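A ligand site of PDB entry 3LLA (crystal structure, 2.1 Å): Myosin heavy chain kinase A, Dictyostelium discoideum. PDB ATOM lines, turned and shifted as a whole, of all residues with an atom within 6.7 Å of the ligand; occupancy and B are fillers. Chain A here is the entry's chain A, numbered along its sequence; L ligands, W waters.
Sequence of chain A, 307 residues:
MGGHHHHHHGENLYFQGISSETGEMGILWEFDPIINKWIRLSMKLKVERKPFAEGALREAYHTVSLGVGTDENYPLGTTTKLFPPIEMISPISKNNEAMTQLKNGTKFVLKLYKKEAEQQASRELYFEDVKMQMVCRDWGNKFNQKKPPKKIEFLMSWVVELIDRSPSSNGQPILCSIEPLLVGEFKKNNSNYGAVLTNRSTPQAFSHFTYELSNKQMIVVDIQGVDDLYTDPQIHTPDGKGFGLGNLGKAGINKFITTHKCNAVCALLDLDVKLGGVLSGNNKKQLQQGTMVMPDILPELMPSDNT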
ATOM      1  N   PHE A  52      -7.772   8.139  21.396  1.00  0.00           N
ATOM      2  CA  PHE A  52      -7.450   6.934  22.176  1.00  0.00           C
ATOM      3  C   PHE A  52      -7.689   5.633  21.389  1.00  0.00           C
ATOM      4  O   PHE A  52      -7.346   4.555  21.859  1.00  0.00           O
ATOM      5  CB  PHE A  52      -8.215   6.910  23.505  1.00  0.00           C
ATOM      6  CG  PHE A  52      -9.700   6.615  23.375  1.00  0.00           C
ATOM      7  CD1 PHE A  52     -10.180   5.291  23.356  1.00  0.00           C
ATOM      8  CD2 PHE A  52     -10.635   7.653  23.307  1.00  0.00           C
ATOM      9  CE1 PHE A  52     -11.547   5.025  23.251  1.00  0.00           C
ATOM     10  CE2 PHE A  52     -12.004   7.395  23.207  1.00  0.00           C
ATOM     11  CZ  PHE A  52     -12.466   6.084  23.170  1.00  0.00           C
ATOM     12  N   ALA A  53      -8.269   5.763  20.206  1.00  0.00           N
ATOM     13  CA  ALA A  53      -8.495   4.612  19.339  1.00  0.00           C
ATOM     14  C   ALA A  53      -8.835   5.078  17.930  1.00  0.00           C
ATOM     15  O   ALA A  53      -9.283   6.215  17.721  1.00  0.00           O
ATOM     16  CB  ALA A  53      -9.602   3.710  19.901  1.00  0.00           C
ATOM     17  N   GLU A  54      -8.615   4.208  16.954  1.00  0.00           N
ATOM     18  CA  GLU A  54      -9.006   4.504  15.587  1.00  0.00           C
ATOM     19  C   GLU A  54      -9.495   3.253  14.867  1.00  0.00           C
ATOM     20  O   GLU A  54      -9.216   2.125  15.284  1.00  0.00           O
ATOM     21  CB  GLU A  54      -7.864   5.183  14.833  1.00  0.00           C
ATOM     22  CG  GLU A  54      -6.728   4.261  14.393  1.00  0.00           C
ATOM     23  CD  GLU A  54      -5.528   5.046  13.860  1.00  0.00           C
ATOM     24  OE1 GLU A  54      -5.233   4.930  12.649  1.00  0.00           O
ATOM     25  OE2 GLU A  54      -4.908   5.791  14.660  1.00  0.00           O
ATOM     26  N   GLY A  55     -10.230   3.466  13.781  1.00  0.00           N
ATOM     27  CA  GLY A  55     -10.661   2.384  12.917  1.00  0.00           C
ATOM     28  C   GLY A  55     -10.299   2.723  11.484  1.00  0.00           C
ATOM     29  O   GLY A  55      -9.522   3.648  11.245  1.00  0.00           O
ATOM     30  N   ALA A  56     -10.875   1.996  10.540  1.00  0.00           N
ATOM     31  CA  ALA A  56     -10.628   2.241   9.116  1.00  0.00           C
ATOM     32  C   ALA A  56     -10.934   3.696   8.706  1.00  0.00           C
ATOM     33  O   ALA A  56     -10.270   4.241   7.824  1.00  0.00           O
ATOM     34  CB  ALA A  56     -11.442   1.256   8.258  1.00  0.00           C
ATOM     35  N   LEU A  57     -11.910   4.312   9.352  1.00  0.00           N
ATOM     36  CA  LEU A  57     -12.453   5.609   8.909  1.00  0.00           C
ATOM     37  C   LEU A  57     -12.281   6.796   9.882  1.00  0.00           C
ATOM     38  O   LEU A  57     -12.042   7.920   9.459  1.00  0.00           O
ATOM     39  CB  LEU A  57     -13.942   5.424   8.576  1.00  0.00           C
ATOM     40  CG  LEU A  57     -14.246   4.605   7.313  1.00  0.00           C
ATOM     41  CD1 LEU A  57     -15.275   3.504   7.568  1.00  0.00           C
ATOM     42  CD2 LEU A  57     -14.698   5.519   6.167  1.00  0.00           C
ATOM     43  N   ARG A  58     -12.417   6.542  11.186  1.00  0.00           N
ATOM     44  CA  ARG A  58     -12.533   7.630  12.151  1.00  0.00           C
ATOM     45  C   ARG A  58     -11.562   7.469  13.317  1.00  0.00           C
ATOM     46  O   ARG A  58     -11.079   6.372  13.589  1.00  0.00           O
ATOM     47  CB  ARG A  58     -13.978   7.715  12.662  1.00  0.00           C
ATOM     48  CG  ARG A  58     -15.013   7.845  11.533  1.00  0.00           C
ATOM     49  CD  ARG A  58     -16.466   7.974  12.023  1.00  0.00           C
ATOM     50  NE  ARG A  58     -16.969   6.758  12.643  1.00  0.00           N
ATOM     51  CZ  ARG A  58     -18.095   6.678  13.360  1.00  0.00           C
ATOM     52  NH1 ARG A  58     -18.876   7.740  13.525  1.00  0.00           N
ATOM     53  NH2 ARG A  58     -18.445   5.513  13.910  1.00  0.00           N
ATOM     54  N   GLU A  59     -11.291   8.569  14.016  1.00  0.00           N
ATOM     55  CA  GLU A  59     -10.576   8.497  15.282  1.00  0.00           C
ATOM     56  C   GLU A  59     -11.498   8.934  16.418  1.00  0.00           C
ATOM     57  O   GLU A  59     -12.346   9.809  16.254  1.00  0.00           O
ATOM     58  CB  GLU A  59      -9.281   9.328  15.240  1.00  0.00           C
ATOM     59  CG  GLU A  59      -8.182   8.673  14.365  1.00  0.00           C
ATOM     60  CD  GLU A  59      -6.962   9.553  14.107  1.00  0.00           C
ATOM     61  OE1 GLU A  59      -7.112  10.802  14.013  1.00  0.00           O
ATOM     62  OE2 GLU A  59      -5.842   8.998  13.978  1.00  0.00           O
ATOM     63  N   ALA A  60     -11.345   8.281  17.568  1.00  0.00           N
ATOM     64  CA  ALA A  60     -12.227   8.493  18.706  1.00  0.00           C
ATOM     65  C   ALA A  60     -11.457   9.180  19.821  1.00  0.00           C
ATOM     66  O   ALA A  60     -10.298   8.861  20.073  1.00  0.00           O
ATOM     67  CB  ALA A  60     -12.805   7.164  19.173  1.00  0.00           C
ATOM     68  N   HIS A  62     -11.522  10.885  23.896  1.00  0.00           N
ATOM     69  CA  HIS A  62     -12.175  11.086  25.183  1.00  0.00           C
ATOM     70  C   HIS A  62     -12.640  12.537  25.301  1.00  0.00           C
ATOM     71  O   HIS A  62     -11.917  13.457  24.930  1.00  0.00           O
ATOM     72  CB  HIS A  62     -11.257  10.762  26.360  1.00  0.00           C
ATOM     73  CG  HIS A  62     -10.908   9.311  26.482  1.00  0.00           C
ATOM     74  ND1 HIS A  62     -11.868   8.328  26.689  1.00  0.00           N
ATOM     75  CD2 HIS A  62      -9.721   8.670  26.424  1.00  0.00           C
ATOM     76  CE1 HIS A  62     -11.274   7.153  26.759  1.00  0.00           C
ATOM     77  NE2 HIS A  62      -9.968   7.327  26.595  1.00  0.00           N
ATOM     78  N   VAL A 109     -17.492   9.985  24.156  1.00  0.00           N
ATOM     79  CA  VAL A 109     -16.612   9.786  23.014  1.00  0.00           C
ATOM     80  C   VAL A 109     -16.997  10.720  21.870  1.00  0.00           C
ATOM     81  O   VAL A 109     -18.186  10.851  21.533  1.00  0.00           O
ATOM     82  CB  VAL A 109     -16.644   8.335  22.521  1.00  0.00           C
ATOM     83  CG1 VAL A 109     -15.769   8.152  21.286  1.00  0.00           C
ATOM     84  CG2 VAL A 109     -16.206   7.383  23.649  1.00  0.00           C
ATOM     85  N   LYS A 111     -16.085  11.375  17.820  1.00  0.00           N
ATOM     86  CA  LYS A 111     -15.493  10.727  16.656  1.00  0.00           C
ATOM     87  C   LYS A 111     -15.397  11.696  15.486  1.00  0.00           C
ATOM     88  O   LYS A 111     -16.376  12.364  15.135  1.00  0.00           O
ATOM     89  CB  LYS A 111     -16.301   9.487  16.242  1.00  0.00           C
ATOM     90  CG  LYS A 111     -16.292   8.364  17.284  1.00  0.00           C
ATOM     91  CD  LYS A 111     -17.079   7.173  16.848  1.00  0.00           C
ATOM     92  CE  LYS A 111     -17.077   6.097  17.927  1.00  0.00           C
ATOM     93  NZ  LYS A 111     -17.936   4.920  17.552  1.00  0.00           N
ATOM     94  N   TYR A 113     -13.854  12.104  11.378  1.00  0.00           N
ATOM     95  CA  TYR A 113     -13.365  11.402  10.198  1.00  0.00           C
ATOM     96  C   TYR A 113     -11.902  11.711   9.939  1.00  0.00           C
ATOM     97  O   TYR A 113     -11.458  12.851  10.092  1.00  0.00           O
ATOM     98  CB  TYR A 113     -14.197  11.744   8.952  1.00  0.00           C
ATOM     99  CG  TYR A 113     -15.487  10.977   8.857  1.00  0.00           C
ATOM    100  CD1 TYR A 113     -16.719  11.604   9.073  1.00  0.00           C
ATOM    101  CD2 TYR A 113     -15.489   9.615   8.567  1.00  0.00           C
ATOM    102  CE1 TYR A 113     -17.907  10.896   8.985  1.00  0.00           C
ATOM    103  CE2 TYR A 113     -16.666   8.904   8.488  1.00  0.00           C
ATOM    104  CZ  TYR A 113     -17.869   9.541   8.694  1.00  0.00           C
ATOM    105  OH  TYR A 113     -19.035   8.822   8.610  1.00  0.00           O
ATOM    106  N   LYS A 114     -11.149  10.669   9.582  1.00  0.00           N
ATOM    107  CA  LYS A 114      -9.754  10.818   9.156  1.00  0.00           C
ATOM    108  C   LYS A 114      -9.678  11.401   7.738  1.00  0.00           C
ATOM    109  O   LYS A 114     -10.698  11.501   7.046  1.00  0.00           O
ATOM    110  CB  LYS A 114      -9.040   9.477   9.226  1.00  0.00           C
ATOM    111  CG  LYS A 114      -8.843   8.960  10.647  1.00  0.00           C
ATOM    112  CD  LYS A 114      -8.028   7.674  10.689  1.00  0.00           C
ATOM    113  CE  LYS A 114      -8.671   6.591   9.849  1.00  0.00           C
ATOM    114  NZ  LYS A 114      -7.963   5.300  10.037  1.00  0.00           N
ATOM    115  N   LEU A 155     -26.331   2.162  21.972  1.00  0.00           N
ATOM    116  CA  LEU A 155     -26.047   3.464  22.538  1.00  0.00           C
ATOM    117  C   LEU A 155     -26.767   4.560  21.736  1.00  0.00           C
ATOM    118  O   LEU A 155     -26.993   4.403  20.529  1.00  0.00           O
ATOM    119  CB  LEU A 155     -24.545   3.755  22.492  1.00  0.00           C
ATOM    120  CG  LEU A 155     -23.514   2.967  23.307  1.00  0.00           C
ATOM    121  CD1 LEU A 155     -22.125   3.593  23.123  1.00  0.00           C
ATOM    122  CD2 LEU A 155     -23.859   2.885  24.783  1.00  0.00           C
ATOM    123  N   GLU A 179     -21.038   9.939  21.306  1.00  0.00           N
ATOM    124  CA  GLU A 179     -21.804   8.828  21.888  1.00  0.00           C
ATOM    125  C   GLU A 179     -21.278   8.518  23.300  1.00  0.00           C
ATOM    126  O   GLU A 179     -20.196   9.007  23.671  1.00  0.00           O
ATOM    127  CB  GLU A 179     -21.713   7.598  20.964  1.00  0.00           C
ATOM    128  CG  GLU A 179     -20.283   7.155  20.618  1.00  0.00           C
ATOM    129  CD  GLU A 179     -20.209   6.012  19.616  1.00  0.00           C
ATOM    130  OE1 GLU A 179     -20.462   6.240  18.413  1.00  0.00           O
ATOM    131  OE2 GLU A 179     -19.858   4.879  20.021  1.00  0.00           O
ATOM    132  N   PRO A 180     -22.009   7.704  24.105  1.00  0.00           N
ATOM    133  CA  PRO A 180     -21.474   7.448  25.442  1.00  0.00           C
ATOM    134  C   PRO A 180     -20.181   6.612  25.393  1.00  0.00           C
ATOM    135  O   PRO A 180     -19.899   5.960  24.377  1.00  0.00           O
ATOM    136  CB  PRO A 180     -22.601   6.675  26.121  1.00  0.00           C
ATOM    137  CG  PRO A 180     -23.855   7.121  25.379  1.00  0.00           C
ATOM    138  CD  PRO A 180     -23.382   7.179  23.965  1.00  0.00           C
ATOM    139  N   LEU A 181     -19.395   6.682  26.464  1.00  0.00           N
ATOM    140  CA  LEU A 181     -18.179   5.900  26.566  1.00  0.00           C
ATOM    141  C   LEU A 181     -18.516   4.461  26.947  1.00  0.00           C
ATOM    142  O   LEU A 181     -19.241   4.216  27.915  1.00  0.00           O
ATOM    143  CB  LEU A 181     -17.227   6.527  27.594  1.00  0.00           C
ATOM    144  CG  LEU A 181     -15.951   5.732  27.990  1.00  0.00           C
ATOM    145  CD1 LEU A 181     -14.941   5.606  26.860  1.00  0.00           C
ATOM    146  CD2 LEU A 181     -15.295   6.344  29.250  1.00  0.00           C
ATOM    147  N   LEU A 182     -18.022   3.502  26.176  1.00  0.00           N
ATOM    148  CA  LEU A 182     -18.132   2.102  26.573  1.00  0.00           C
ATOM    149  C   LEU A 182     -16.945   1.708  27.431  1.00  0.00           C
ATOM    150  O   LEU A 182     -15.807   2.004  27.101  1.00  0.00           O
ATOM    151  CB  LEU A 182     -18.224   1.182  25.368  1.00  0.00           C
ATOM    152  CG  LEU A 182     -19.476   1.306  24.500  1.00  0.00           C
ATOM    153  CD1 LEU A 182     -19.266   0.667  23.124  1.00  0.00           C
ATOM    154  CD2 LEU A 182     -20.688   0.730  25.214  1.00  0.00           C
ATOM    155  N   VAL A 183     -17.206   1.034  28.538  1.00  0.00           N
ATOM    156  CA  VAL A 183     -16.139   0.581  29.447  1.00  0.00           C
ATOM    157  C   VAL A 183     -16.026  -0.937  29.391  1.00  0.00           C
ATOM    158  O   VAL A 183     -16.992  -1.647  29.686  1.00  0.00           O
ATOM    159  CB  VAL A 183     -16.381   1.067  30.905  1.00  0.00           C
ATOM    160  CG1 VAL A 183     -15.365   0.452  31.882  1.00  0.00           C
ATOM    161  CG2 VAL A 183     -16.339   2.580  30.973  1.00  0.00           C
ATOM    162  N   GLY A 184     -14.854  -1.428  28.993  1.00  0.00           N
ATOM    163  CA  GLY A 184     -14.604  -2.870  28.882  1.00  0.00           C
ATOM    164  C   GLY A 184     -13.919  -3.193  27.572  1.00  0.00           C
ATOM    165  O   GLY A 184     -13.411  -2.313  26.875  1.00  0.00           O
ATOM    166  N   PHE A 186     -13.849  -4.008  23.832  1.00  0.00           N
ATOM    167  CA  PHE A 186     -14.642  -3.711  22.638  1.00  0.00           C
ATOM    168  C   PHE A 186     -14.439  -4.785  21.589  1.00  0.00           C
ATOM    169  O   PHE A 186     -13.315  -5.006  21.147  1.00  0.00           O
ATOM    170  CB  PHE A 186     -14.215  -2.345  22.059  1.00  0.00           C
ATOM    171  CG  PHE A 186     -15.186  -1.762  21.026  1.00  0.00           C
ATOM    172  CD1 PHE A 186     -16.022  -0.707  21.377  1.00  0.00           C
ATOM    173  CD2 PHE A 186     -15.232  -2.262  19.720  1.00  0.00           C
ATOM    174  CE1 PHE A 186     -16.903  -0.162  20.438  1.00  0.00           C
ATOM    175  CE2 PHE A 186     -16.111  -1.725  18.777  1.00  0.00           C
ATOM    176  CZ  PHE A 186     -16.948  -0.666  19.141  1.00  0.00           C
ATOM    177  N   LYS A 188     -15.970  -6.721  17.865  1.00  0.00           N
ATOM    178  CA  LYS A 188     -16.809  -6.736  16.681  1.00  0.00           C
ATOM    179  C   LYS A 188     -17.246  -8.165  16.385  1.00  0.00           C
ATOM    180  O   LYS A 188     -16.405  -9.045  16.241  1.00  0.00           O
ATOM    181  CB  LYS A 188     -16.029  -6.138  15.506  1.00  0.00           C
ATOM    182  CG  LYS A 188     -16.810  -5.977  14.227  1.00  0.00           C
ATOM    183  CD  LYS A 188     -15.932  -5.214  13.243  1.00  0.00           C
ATOM    184  CE  LYS A 188     -16.643  -4.994  11.941  1.00  0.00           C
ATOM    185  NZ  LYS A 188     -16.138  -3.728  11.335  1.00  0.00           N
ATOM    186  N   ASP A 222     -22.811  -5.291  11.338  1.00  0.00           N
ATOM    187  CA  ASP A 222     -21.764  -4.556  12.048  1.00  0.00           C
ATOM    188  C   ASP A 222     -22.074  -4.484  13.568  1.00  0.00           C
ATOM    189  O   ASP A 222     -21.961  -3.418  14.199  1.00  0.00           O
ATOM    190  CB  ASP A 222     -21.559  -3.146  11.451  1.00  0.00           C
ATOM    191  CG  ASP A 222     -20.218  -2.965  10.718  1.00  0.00           C
ATOM    192  OD1 ASP A 222     -19.347  -3.873  10.760  1.00  0.00           O
ATOM    193  OD2 ASP A 222     -20.015  -1.891  10.102  1.00  0.00           O
ATOM    194  N   GLN A 224     -21.305  -4.608  17.064  1.00  0.00           N
ATOM    195  CA  GLN A 224     -20.074  -4.460  17.806  1.00  0.00           C
ATOM    196  C   GLN A 224     -20.274  -3.605  19.044  1.00  0.00           C
ATOM    197  O   GLN A 224     -21.200  -2.774  19.105  1.00  0.00           O
ATOM    198  CB  GLN A 224     -19.022  -3.806  16.924  1.00  0.00           C
ATOM    199  CG  GLN A 224     -19.363  -2.392  16.474  1.00  0.00           C
ATOM    200  CD  GLN A 224     -18.481  -1.964  15.345  1.00  0.00           C
ATOM    201  OE1 GLN A 224     -17.260  -2.139  15.415  1.00  0.00           O
ATOM    202  NE2 GLN A 224     -19.068  -1.427  14.299  1.00  0.00           N
ATOM    203  N   VAL A 226     -19.324  -3.453  23.622  1.00  0.00           N
ATOM    204  CA  VAL A 226     -18.871  -4.124  24.851  1.00  0.00           C
ATOM    205  C   VAL A 226     -20.056  -4.872  25.425  1.00  0.00           C
ATOM    206  O   VAL A 226     -21.077  -4.276  25.759  1.00  0.00           O
ATOM    207  CB  VAL A 226     -18.271  -3.113  25.874  1.00  0.00           C
ATOM    208  CG1 VAL A 226     -17.978  -3.780  27.238  1.00  0.00           C
ATOM    209  CG2 VAL A 226     -17.029  -2.459  25.300  1.00  0.00           C
ATOM    210  N   THR A 231     -22.661  -0.305  19.424  1.00  0.00           N
ATOM    211  CA  THR A 231     -22.518   0.987  18.750  1.00  0.00           C
ATOM    212  C   THR A 231     -22.027   0.818  17.294  1.00  0.00           C
ATOM    213  O   THR A 231     -21.662  -0.281  16.884  1.00  0.00           O
ATOM    214  CB  THR A 231     -21.614   1.967  19.561  1.00  0.00           C
ATOM    215  OG1 THR A 231     -21.790   3.307  19.063  1.00  0.00           O
ATOM    216  CG2 THR A 231     -20.124   1.571  19.483  1.00  0.00           C
ATOM    217  N   ASP A 232     -22.115   1.901  16.512  1.00  0.00           N
ATOM    218  CA  ASP A 232     -21.671   1.894  15.102  1.00  0.00           C
ATOM    219  C   ASP A 232     -22.183   0.701  14.269  1.00  0.00           C
ATOM    220  O   ASP A 232     -21.413   0.032  13.596  1.00  0.00           O
ATOM    221  CB  ASP A 232     -20.126   1.993  15.041  1.00  0.00           C
ATOM    222  CG  ASP A 232     -19.587   2.135  13.619  1.00  0.00           C
ATOM    223  OD1 ASP A 232     -20.174   2.877  12.808  1.00  0.00           O
ATOM    224  OD2 ASP A 232     -18.539   1.501  13.319  1.00  0.00           O
HETATM  225  P1  LIG L   1     -14.150   0.486  12.367  1.00  0.00           P
HETATM  226  O1  LIG L   1     -13.392   0.494  11.065  1.00  0.00           O
HETATM  227  O2  LIG L   1     -13.271   0.795  13.554  1.00  0.00           O
HETATM  228  O3  LIG L   1     -14.997  -0.732  12.595  1.00  0.00           O
HETATM  229  P2  LIG L   1     -14.711   3.510  12.340  1.00  0.00           P
HETATM  230  O4  LIG L   1     -13.475   3.699  11.499  1.00  0.00           O
HETATM  231  O5  LIG L   1     -15.840   4.466  12.070  1.00  0.00           O
HETATM  232  C1  LIG L   1     -15.373   1.822  12.218  1.00  0.00           C
HETATM  233  P3  LIG L   1     -15.083   3.423  15.137  1.00  0.00           P
HETATM  234  O6  LIG L   1     -15.174   1.928  15.232  1.00  0.00           O
HETATM  235  O7  LIG L   1     -16.367   4.210  15.194  1.00  0.00           O
HETATM  236  O8  LIG L   1     -14.220   3.822  13.847  1.00  0.00           O
HETATM  237  O9  LIG L   1     -14.096   3.869  16.316  1.00  0.00           O
HETATM  238  C2  LIG L   1     -12.780   3.316  16.346  1.00  0.00           C
HETATM  239  C3  LIG L   1     -12.535   2.504  17.604  1.00  0.00           C
HETATM  240  O10 LIG L   1     -12.859   3.247  18.799  1.00  0.00           O
HETATM  241  C4  LIG L   1     -13.356   1.231  17.709  1.00  0.00           C
HETATM  242  O11 LIG L   1     -12.805   0.129  16.981  1.00  0.00           O
HETATM  243  C5  LIG L   1     -13.331   0.953  19.186  1.00  0.00           C
HETATM  244  O12 LIG L   1     -12.037   0.455  19.510  1.00  0.00           O
HETATM  245  C6  LIG L   1     -13.387   2.340  19.792  1.00  0.00           C
HETATM  246  N1  LIG L   1     -14.751   2.817  20.159  1.00  0.00           N
HETATM  247  C7  LIG L   1     -15.755   3.156  19.308  1.00  0.00           C
HETATM  248  N2  LIG L   1     -16.862   3.599  19.980  1.00  0.00           N
HETATM  249  C8  LIG L   1     -16.562   3.576  21.287  1.00  0.00           C
HETATM  250  C9  LIG L   1     -17.269   3.910  22.548  1.00  0.00           C
HETATM  251  N3  LIG L   1     -18.531   4.385  22.528  1.00  0.00           N
HETATM  252  N4  LIG L   1     -16.601   3.733  23.696  1.00  0.00           N
HETATM  253  C10 LIG L   1     -15.338   3.261  23.752  1.00  0.00           C
HETATM  254  N5  LIG L   1     -14.629   2.936  22.643  1.00  0.00           N
HETATM  255  C11 LIG L   1     -15.169   3.065  21.410  1.00  0.00           C
HETATM  256  O   HOH W   1     -12.737   1.262  23.604  1.00  0.00           O
HETATM  257  O   HOH W   2     -11.324   0.026  21.907  1.00  0.00           O
HETATM  258  O   HOH W   3     -18.320   1.994  10.471  1.00  0.00           O
HETATM  259  O   HOH W   4     -10.214  -0.245  16.011  1.00  0.00           O
HETATM  260  O   HOH W   5     -14.910  -0.867  15.153  1.00  0.00           O
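O4 of the ligand lies within hydrogen-bond range of N of Arg 58 (3.0 Å). O5 of the ligand is in salt-bridge range of NE of Arg 58. N of Leu 57 sits at hydrogen-bond distance from O4 of the ligand (2.7 Å). N3 of the ligand lies within hydrogen-bond range of O of Pro 180 (2.8 Å). The backbone NH (N) of Leu 182 sits at hydrogen-bond distance from a nitrogen (N4) of the ligand (2.9 Å). A nitrogen (N3) of the ligand lies within hydrogen-bond range of the side-chain carboxylate (OE2) of Glu 179, 2.9 Å away. NZ of Lys 111 is in salt-bridge range of O7 of the ligand. An oxygen (O1) of the ligand is in hydrogen-bond range of the backbone NH (N) of Ala 56. An oxygen (O3) of the ligand is in salt-bridge range of the side-chain amino group (NZ) of Lys 188 (3.4 Å).
The side-chain carboxylate (OD1) of Asp 232 lies within salt-bridge range of the guanidinium group (NH2) of Arg 58 (3.3 Å). The side-chain carboxylate of Glu 179 lies within salt-bridge range of the side-chain amino group of Lys 111 (3.0 Å). The side-chain carboxylate (OE2) of Glu 179 lies within hydrogen-bond range of the side-chain hydroxyl (OG1) of Thr 231, 2.7 Å away. The backbone carbonyl oxygen (O) of Asp 232 sits at hydrogen-bond distance from the side-chain amide nitrogen (NE2) of Gln 224. OD1 of Asp 222 is in salt-bridge range of NZ of Lys 188 (3.3 Å). O of Ala 53 sits at hydrogen-bond distance from N of Ala 60 (2.9 Å). The side-chain carboxylate (OE1) of Glu 54 lies within salt-bridge range of the side-chain amino group (NZ) of Lys 114, 3.8 Å away. The backbone NH (N) of Thr 231 lies within hydrogen-bond range of the backbone carbonyl oxygen (O) of Gln 224 (2.9 Å).
CE1 of Phe 52 touches N5 of the ligand, at 3.8 Å. Ala 53 touches the ligand (CB to O10, 3.5 Å). C of Glu 54 touches C2 of the ligand (3.6 Å). CA of Gly 55 touches O2 of the ligand (3.1 Å). Ala 60 touches the ligand (CB to O10, 3.9 Å). Val 109 touches the ligand (CG2 to N4, 3.7 Å). Leu 155 touches the ligand. Leu 181 touches the ligand (C to N4, 3.8 Å). Phe 186 touches the ligand (CE1 to N1, 3.7 Å). OE1 of Gln 224 touches O3 of the ligand (3.9 Å). Thr 231 touches the ligand. Asp 232 touches the ligand. Of the 28 residues printed, 20 come within 4 Å of the ligand. The nearest printed residue that does not touch the ligand is Val 183 (5.6 Å).
Water W5 lies within hydrogen-bond range of an oxygen (O3) of the ligand (2.6 Å) and the side-chain amide oxygen of Gln 224 (2.7 Å). Water W4 bridges the backbone carbonyl oxygen of Glu 54 (2.7 Å) and an oxygen (O11) of the ligand (2.8 Å).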
